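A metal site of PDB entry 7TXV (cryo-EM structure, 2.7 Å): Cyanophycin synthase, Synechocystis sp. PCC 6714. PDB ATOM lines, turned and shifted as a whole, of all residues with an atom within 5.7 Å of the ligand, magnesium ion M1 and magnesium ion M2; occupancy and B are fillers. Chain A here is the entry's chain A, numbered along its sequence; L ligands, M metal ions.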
ATOM      1  N   GLY A 495       0.947  30.778 -33.553  1.00  0.00           N
ATOM      2  CA  GLY A 495      -0.064  29.754 -33.775  1.00  0.00           C
ATOM      3  C   GLY A 495      -1.216  29.948 -32.823  1.00  0.00           C
ATOM      4  O   GLY A 495      -1.071  30.658 -31.821  1.00  0.00           O
ATOM      5  N   THR A 496      -2.362  29.368 -33.088  1.00  0.00           N
ATOM      6  CA  THR A 496      -3.505  29.555 -32.206  1.00  0.00           C
ATOM      7  C   THR A 496      -3.310  29.013 -30.800  1.00  0.00           C
ATOM      8  O   THR A 496      -3.659  29.699 -29.839  1.00  0.00           O
ATOM      9  CB  THR A 496      -4.807  28.992 -32.794  1.00  0.00           C
ATOM     10  OG1 THR A 496      -5.127  29.666 -34.023  1.00  0.00           O
ATOM     11  CG2 THR A 496      -5.917  29.259 -31.850  1.00  0.00           C
ATOM     12  N   ASN A 497      -2.760  27.815 -30.649  1.00  0.00           N
ATOM     13  CA  ASN A 497      -2.530  27.211 -29.324  1.00  0.00           C
ATOM     14  C   ASN A 497      -1.131  26.671 -29.153  1.00  0.00           C
ATOM     15  O   ASN A 497      -0.561  26.106 -30.085  1.00  0.00           O
ATOM     16  CB  ASN A 497      -3.471  26.062 -29.086  1.00  0.00           C
ATOM     17  CG  ASN A 497      -4.850  26.389 -29.023  1.00  0.00           C
ATOM     18  OD1 ASN A 497      -5.305  27.011 -28.074  1.00  0.00           O
ATOM     19  ND2 ASN A 497      -5.590  25.968 -30.004  1.00  0.00           N
ATOM     20  N   GLY A 498      -0.591  26.761 -27.937  1.00  0.00           N
ATOM     21  CA  GLY A 498       0.703  26.170 -27.583  1.00  0.00           C
ATOM     22  C   GLY A 498       1.939  27.045 -27.653  1.00  0.00           C
ATOM     23  O   GLY A 498       3.051  26.582 -27.374  1.00  0.00           O
ATOM     24  N   LYS A 499       1.755  28.322 -27.937  1.00  0.00           N
ATOM     25  CA  LYS A 499       2.853  29.270 -28.037  1.00  0.00           C
ATOM     26  C   LYS A 499       3.666  29.437 -26.774  1.00  0.00           C
ATOM     27  O   LYS A 499       4.897  29.448 -26.842  1.00  0.00           O
ATOM     28  CB  LYS A 499       2.345  30.634 -28.382  1.00  0.00           C
ATOM     29  CG  LYS A 499       1.756  30.807 -29.710  1.00  0.00           C
ATOM     30  CD  LYS A 499       1.416  32.298 -29.967  1.00  0.00           C
ATOM     31  CE  LYS A 499       0.220  32.795 -29.243  1.00  0.00           C
ATOM     32  NZ  LYS A 499      -0.958  32.244 -29.806  1.00  0.00           N
ATOM     33  N   THR A 500       3.018  29.555 -25.632  1.00  0.00           N
ATOM     34  CA  THR A 500       3.726  29.787 -24.375  1.00  0.00           C
ATOM     35  C   THR A 500       4.550  28.592 -23.977  1.00  0.00           C
ATOM     36  O   THR A 500       5.668  28.730 -23.500  1.00  0.00           O
ATOM     37  CB  THR A 500       2.781  30.218 -23.250  1.00  0.00           C
ATOM     38  OG1 THR A 500       2.126  31.467 -23.602  1.00  0.00           O
ATOM     39  CG2 THR A 500       3.517  30.394 -21.960  1.00  0.00           C
ATOM     40  N   THR A 501       3.996  27.398 -24.148  1.00  0.00           N
ATOM     41  CA  THR A 501       4.691  26.185 -23.798  1.00  0.00           C
ATOM     42  C   THR A 501       5.908  25.958 -24.685  1.00  0.00           C
ATOM     43  O   THR A 501       6.983  25.600 -24.187  1.00  0.00           O
ATOM     44  CB  THR A 501       3.737  24.983 -23.921  1.00  0.00           C
ATOM     45  OG1 THR A 501       2.627  25.157 -23.032  1.00  0.00           O
ATOM     46  CG2 THR A 501       4.470  23.727 -23.536  1.00  0.00           C
ATOM     47  N   SER A 521       6.663  36.280 -23.079  1.00  0.00           N
ATOM     48  CA  SER A 521       5.471  35.465 -23.079  1.00  0.00           C
ATOM     49  C   SER A 521       4.277  36.199 -22.540  1.00  0.00           C
ATOM     50  O   SER A 521       4.354  37.362 -22.127  1.00  0.00           O
ATOM     51  CB  SER A 521       5.661  34.256 -22.214  1.00  0.00           C
ATOM     52  OG  SER A 521       5.642  34.604 -20.849  1.00  0.00           O
ATOM     53  N   THR A 522       3.156  35.508 -22.506  1.00  0.00           N
ATOM     54  CA  THR A 522       1.941  36.029 -21.913  1.00  0.00           C
ATOM     55  C   THR A 522       1.976  36.064 -20.377  1.00  0.00           C
ATOM     56  O   THR A 522       1.040  36.559 -19.752  1.00  0.00           O
ATOM     57  CB  THR A 522       0.666  35.326 -22.448  1.00  0.00           C
ATOM     58  OG1 THR A 522       0.791  33.879 -22.389  1.00  0.00           O
ATOM     59  CG2 THR A 522       0.373  35.765 -23.812  1.00  0.00           C
ATOM     60  N   THR A 538       3.283  40.013 -24.556  1.00  0.00           N
ATOM     61  CA  THR A 538       3.465  39.733 -25.959  1.00  0.00           C
ATOM     62  C   THR A 538       3.316  41.046 -26.726  1.00  0.00           C
ATOM     63  O   THR A 538       2.816  42.044 -26.206  1.00  0.00           O
ATOM     64  CB  THR A 538       2.494  38.678 -26.453  1.00  0.00           C
ATOM     65  OG1 THR A 538       1.130  39.098 -26.321  1.00  0.00           O
ATOM     66  CG2 THR A 538       2.697  37.485 -25.726  1.00  0.00           C
ATOM     67  N   GLU A 558       7.216  34.882 -28.052  1.00  0.00           N
ATOM     68  CA  GLU A 558       5.925  34.322 -28.500  1.00  0.00           C
ATOM     69  C   GLU A 558       5.210  35.483 -29.158  1.00  0.00           C
ATOM     70  O   GLU A 558       5.184  36.584 -28.624  1.00  0.00           O
ATOM     71  CB  GLU A 558       5.050  33.646 -27.398  1.00  0.00           C
ATOM     72  CG  GLU A 558       3.969  34.456 -26.704  1.00  0.00           C
ATOM     73  CD  GLU A 558       3.089  33.692 -25.574  1.00  0.00           C
ATOM     74  OE1 GLU A 558       3.610  33.391 -24.540  1.00  0.00           O
ATOM     75  OE2 GLU A 558       1.868  33.465 -25.716  1.00  0.00           O
ATOM     76  N   ASN A 581      -0.166  26.018 -35.417  1.00  0.00           N
ATOM     77  CA  ASN A 581      -1.515  25.625 -35.827  1.00  0.00           C
ATOM     78  C   ASN A 581      -2.383  26.818 -36.161  1.00  0.00           C
ATOM     79  O   ASN A 581      -2.123  27.932 -35.710  1.00  0.00           O
ATOM     80  CB  ASN A 581      -2.143  24.754 -34.751  1.00  0.00           C
ATOM     81  CG  ASN A 581      -2.083  25.348 -33.415  1.00  0.00           C
ATOM     82  OD1 ASN A 581      -2.697  26.357 -33.115  1.00  0.00           O
ATOM     83  ND2 ASN A 581      -1.308  24.756 -32.576  1.00  0.00           N
ATOM     84  N   ASP A 585     -10.705  30.078 -33.245  1.00  0.00           N
ATOM     85  CA  ASP A 585     -10.658  30.601 -31.906  1.00  0.00           C
ATOM     86  C   ASP A 585     -10.303  32.064 -32.028  1.00  0.00           C
ATOM     87  O   ASP A 585      -9.304  32.398 -32.657  1.00  0.00           O
ATOM     88  CB  ASP A 585      -9.653  29.847 -31.044  1.00  0.00           C
ATOM     89  CG  ASP A 585      -9.647  30.341 -29.627  1.00  0.00           C
ATOM     90  OD1 ASP A 585     -10.332  31.279 -29.286  1.00  0.00           O
ATOM     91  OD2 ASP A 585      -8.843  29.991 -28.789  1.00  0.00           O
ATOM     92  N   HIS A 586     -11.169  32.931 -31.521  1.00  0.00           N
ATOM     93  CA  HIS A 586     -11.066  34.387 -31.643  1.00  0.00           C
ATOM     94  C   HIS A 586     -11.434  34.887 -33.033  1.00  0.00           C
ATOM     95  O   HIS A 586     -11.006  35.971 -33.440  1.00  0.00           O
ATOM     96  CB  HIS A 586      -9.637  34.888 -31.347  1.00  0.00           C
ATOM     97  CG  HIS A 586      -9.116  34.435 -30.044  1.00  0.00           C
ATOM     98  ND1 HIS A 586      -9.580  34.930 -28.849  1.00  0.00           N
ATOM     99  CD2 HIS A 586      -8.182  33.519 -29.744  1.00  0.00           C
ATOM    100  CE1 HIS A 586      -8.948  34.351 -27.862  1.00  0.00           C
ATOM    101  NE2 HIS A 586      -8.100  33.453 -28.360  1.00  0.00           N
ATOM    102  N   PHE A 692      -0.738  16.764 -27.753  1.00  0.00           N
ATOM    103  CA  PHE A 692      -0.339  18.107 -28.069  1.00  0.00           C
ATOM    104  C   PHE A 692       0.931  18.515 -27.342  1.00  0.00           C
ATOM    105  O   PHE A 692       1.585  19.467 -27.755  1.00  0.00           O
ATOM    106  CB  PHE A 692      -1.452  19.105 -27.820  1.00  0.00           C
ATOM    107  CG  PHE A 692      -1.955  19.209 -26.449  1.00  0.00           C
ATOM    108  CD1 PHE A 692      -1.299  19.910 -25.498  1.00  0.00           C
ATOM    109  CD2 PHE A 692      -3.126  18.639 -26.124  1.00  0.00           C
ATOM    110  CE1 PHE A 692      -1.783  20.017 -24.254  1.00  0.00           C
ATOM    111  CE2 PHE A 692      -3.611  18.746 -24.880  1.00  0.00           C
ATOM    112  CZ  PHE A 692      -2.938  19.442 -23.932  1.00  0.00           C
ATOM    113  N   MET A 693       1.308  17.792 -26.282  1.00  0.00           N
ATOM    114  CA  MET A 693       2.513  18.127 -25.568  1.00  0.00           C
ATOM    115  C   MET A 693       3.662  17.546 -26.355  1.00  0.00           C
ATOM    116  O   MET A 693       4.754  18.107 -26.392  1.00  0.00           O
ATOM    117  CB  MET A 693       2.460  17.590 -24.167  1.00  0.00           C
ATOM    118  CG  MET A 693       1.424  18.239 -23.301  1.00  0.00           C
ATOM    119  SD  MET A 693       1.624  20.021 -23.100  1.00  0.00           S
ATOM    120  CE  MET A 693       2.938  20.141 -21.949  1.00  0.00           C
ATOM    121  N   ASN A 696       4.280  19.917 -29.279  1.00  0.00           N
ATOM    122  CA  ASN A 696       5.015  21.102 -28.889  1.00  0.00           C
ATOM    123  C   ASN A 696       6.475  20.798 -28.667  1.00  0.00           C
ATOM    124  O   ASN A 696       7.340  21.599 -29.038  1.00  0.00           O
ATOM    125  CB  ASN A 696       4.397  21.698 -27.662  1.00  0.00           C
ATOM    126  CG  ASN A 696       3.134  22.309 -27.977  1.00  0.00           C
ATOM    127  OD1 ASN A 696       2.915  22.790 -29.080  1.00  0.00           O
ATOM    128  ND2 ASN A 696       2.260  22.282 -27.070  1.00  0.00           N
ATOM    129  N   ARG A 731      -1.944  24.553 -14.151  1.00  0.00           N
ATOM    130  CA  ARG A 731      -1.929  24.066 -15.532  1.00  0.00           C
ATOM    131  C   ARG A 731      -1.522  22.588 -15.658  1.00  0.00           C
ATOM    132  O   ARG A 731      -0.321  22.286 -15.610  1.00  0.00           O
ATOM    133  CB  ARG A 731      -0.980  24.865 -16.424  1.00  0.00           C
ATOM    134  CG  ARG A 731      -1.286  26.365 -16.705  1.00  0.00           C
ATOM    135  CD  ARG A 731      -0.309  26.878 -17.776  1.00  0.00           C
ATOM    136  NE  ARG A 731      -0.541  28.280 -18.256  1.00  0.00           N
ATOM    137  CZ  ARG A 731       0.074  29.447 -17.835  1.00  0.00           C
ATOM    138  NH1 ARG A 731       0.988  29.492 -16.907  1.00  0.00           N
ATOM    139  NH2 ARG A 731      -0.229  30.592 -18.415  1.00  0.00           N
ATOM    140  N   MET A 732      -2.484  21.682 -15.852  1.00  0.00           N
ATOM    141  CA  MET A 732      -2.219  20.244 -16.044  1.00  0.00           C
ATOM    142  C   MET A 732      -1.333  19.565 -14.991  1.00  0.00           C
ATOM    143  O   MET A 732      -0.235  19.100 -15.302  1.00  0.00           O
ATOM    144  CB  MET A 732      -1.544  20.053 -17.410  1.00  0.00           C
ATOM    145  CG  MET A 732      -2.423  20.403 -18.600  1.00  0.00           C
ATOM    146  SD  MET A 732      -1.557  20.333 -20.206  1.00  0.00           S
ATOM    147  CE  MET A 732      -1.264  18.575 -20.441  1.00  0.00           C
ATOM    148  N   ASP A 745      -6.709  20.057 -13.159  1.00  0.00           N
ATOM    149  CA  ASP A 745      -6.633  21.212 -14.020  1.00  0.00           C
ATOM    150  C   ASP A 745      -7.850  22.058 -13.750  1.00  0.00           C
ATOM    151  O   ASP A 745      -8.673  21.688 -12.924  1.00  0.00           O
ATOM    152  CB  ASP A 745      -6.545  20.744 -15.486  1.00  0.00           C
ATOM    153  CG  ASP A 745      -5.882  21.739 -16.399  1.00  0.00           C
ATOM    154  OD1 ASP A 745      -5.982  22.907 -16.117  1.00  0.00           O
ATOM    155  OD2 ASP A 745      -5.214  21.346 -17.316  1.00  0.00           O
ATOM    156  N   ARG A 754     -12.118  19.495 -21.877  1.00  0.00           N
ATOM    157  CA  ARG A 754     -11.412  18.852 -22.974  1.00  0.00           C
ATOM    158  C   ARG A 754      -9.941  18.699 -22.622  1.00  0.00           C
ATOM    159  O   ARG A 754      -9.329  17.656 -22.887  1.00  0.00           O
ATOM    160  CB  ARG A 754     -11.569  19.680 -24.231  1.00  0.00           C
ATOM    161  CG  ARG A 754     -10.947  19.136 -25.481  1.00  0.00           C
ATOM    162  CD  ARG A 754     -11.289  19.988 -26.635  1.00  0.00           C
ATOM    163  NE  ARG A 754     -10.754  21.343 -26.468  1.00  0.00           N
ATOM    164  CZ  ARG A 754     -11.173  22.452 -27.126  1.00  0.00           C
ATOM    165  NH1 ARG A 754     -12.138  22.380 -28.025  1.00  0.00           N
ATOM    166  NH2 ARG A 754     -10.592  23.619 -26.878  1.00  0.00           N
ATOM    167  N   ALA A 755      -9.412  19.682 -21.894  1.00  0.00           N
ATOM    168  CA  ALA A 755      -8.020  19.672 -21.522  1.00  0.00           C
ATOM    169  C   ALA A 755      -7.623  18.372 -20.841  1.00  0.00           C
ATOM    170  O   ALA A 755      -6.496  17.917 -21.049  1.00  0.00           O
ATOM    171  CB  ALA A 755      -7.717  20.828 -20.576  1.00  0.00           C
HETATM  172  P1  LIG L   1      -2.554  32.397 -25.157  1.00  0.00           P
HETATM  173  O1  LIG L   1      -1.158  32.873 -24.716  1.00  0.00           O
HETATM  174  O2  LIG L   1      -3.632  32.961 -24.177  1.00  0.00           O
HETATM  175  O3  LIG L   1      -2.944  32.981 -26.557  1.00  0.00           O
HETATM  176  P2  LIG L   1      -1.280  30.077 -25.456  1.00  0.00           P
HETATM  177  O4  LIG L   1      -0.968  30.368 -26.848  1.00  0.00           O
HETATM  178  O5  LIG L   1      -0.088  30.759 -24.599  1.00  0.00           O
HETATM  179  O6  LIG L   1      -2.675  30.795 -25.082  1.00  0.00           O
HETATM  180  P3  LIG L   1      -0.980  27.898 -23.864  1.00  0.00           P
HETATM  181  O7  LIG L   1      -0.686  28.952 -22.887  1.00  0.00           O
HETATM  182  O8  LIG L   1       0.312  27.007 -23.882  1.00  0.00           O
HETATM  183  O9  LIG L   1      -1.304  28.480 -25.325  1.00  0.00           O
HETATM  184  O10 LIG L   1      -2.203  27.044 -23.264  1.00  0.00           O
HETATM  185  C1  LIG L   1      -3.196  26.514 -24.208  1.00  0.00           C
HETATM  186  C2  LIG L   1      -4.099  25.530 -23.447  1.00  0.00           C
HETATM  187  O11 LIG L   1      -5.051  24.968 -24.389  1.00  0.00           O
HETATM  188  C3  LIG L   1      -3.324  24.346 -22.796  1.00  0.00           C
HETATM  189  O12 LIG L   1      -3.504  24.345 -21.376  1.00  0.00           O
HETATM  190  C4  LIG L   1      -4.004  23.079 -23.319  1.00  0.00           C
HETATM  191  O13 LIG L   1      -4.764  22.548 -22.205  1.00  0.00           O
HETATM  192  C5  LIG L   1      -4.890  23.531 -24.524  1.00  0.00           C
HETATM  193  N1  LIG L   1      -4.346  23.182 -25.881  1.00  0.00           N
HETATM  194  C6  LIG L   1      -5.085  22.813 -26.987  1.00  0.00           C
HETATM  195  N2  LIG L   1      -4.345  22.589 -28.044  1.00  0.00           N
HETATM  196  C7  LIG L   1      -3.062  22.804 -27.699  1.00  0.00           C
HETATM  197  C8  LIG L   1      -1.799  22.717 -28.390  1.00  0.00           C
HETATM  198  N3  LIG L   1      -1.750  22.395 -29.700  1.00  0.00           N
HETATM  199  N4  LIG L   1      -0.631  22.966 -27.689  1.00  0.00           N
HETATM  200  C9  LIG L   1      -0.669  23.321 -26.364  1.00  0.00           C
HETATM  201  N5  LIG L   1      -1.824  23.439 -25.692  1.00  0.00           N
HETATM  202  C10 LIG L   1      -3.041  23.190 -26.306  1.00  0.00           C
HETATM  203 MG    MG M   1       0.731  32.851 -24.364  1.00  0.00          MG
HETATM  204 MG    MG M   2      -4.900  33.039 -28.081  1.00  0.00          MG
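An oxygen (O5) of the ligand lies close to the backbone NH of Thr 500.
ND2 of Asn 696 lies within hydrogen-bond range of N4 of the ligand (3.0 Å).
OG1 of Thr 501 lies within hydrogen-bond range of O8 of the ligand (3.1 Å).
N of Gly 498 lies within hydrogen-bond range of O9 of the ligand (3.2 Å).
NZ of Lys 499 is in salt-bridge range of O4 of the ligand (3.5 Å).
O of Phe 692 lies within hydrogen-bond range of ND2 of Asn 696 (3.0 Å).
NE2 of His 586 sits close to OD1 of Asp 585 (3.3 Å).
The side-chain amino group (NZ) of Lys 499 sits at hydrogen-bond distance from the backbone carbonyl oxygen (O) of Gly 495 (2.6 Å).
The backbone NH (N) of Asn 497 sits at hydrogen-bond distance from the side-chain amide oxygen (OD1) of Asn 581 (2.9 Å).
N of Thr 496 is in hydrogen-bond range of O of Asn 581.
Merely in contact with the ligand: Asn 497 (3.6 Å), Asn 581 (3.7 Å), Phe 692 (3.6 Å) and Ala 755 (3.8 Å).
Along chain A the residues within 4 Å of the ligand span positions 497 to 755.
The nearest printed residue that does not touch the ligand is Thr 496 (4.1 Å).
Three residues have an atom within 4 Å of magnesium ion M1: Thr 500, Thr 522 and Glu 558.
The nearest printed residue that does not touch magnesium ion M1 is Lys 499 (4.9 Å).
Merely in contact with magnesium ion M2: His 586 and Thr 496.
The nearest printed residue that does not touch magnesium ion M2 is Lys 499 (4.4 Å).
Magnesium ion M1 is bound by the side-chain carboxylate (OE2) of Glu 558 (1.9 Å), an oxygen (O1) of the ligand (1.9 Å), the side-chain hydroxyl (OG1) of Thr 500 (2.1 Å), the side-chain hydroxyl (OG1) of Thr 522 (2.2 Å) and an oxygen (O5) of the ligand (2.3 Å).
Magnesium ion M1 has five donor atoms within binding distance.
Magnesium ion M2 is bound by O3 of the ligand, 2.5 Å away.
Magnesium ion M2 has one donor atom within binding distance.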
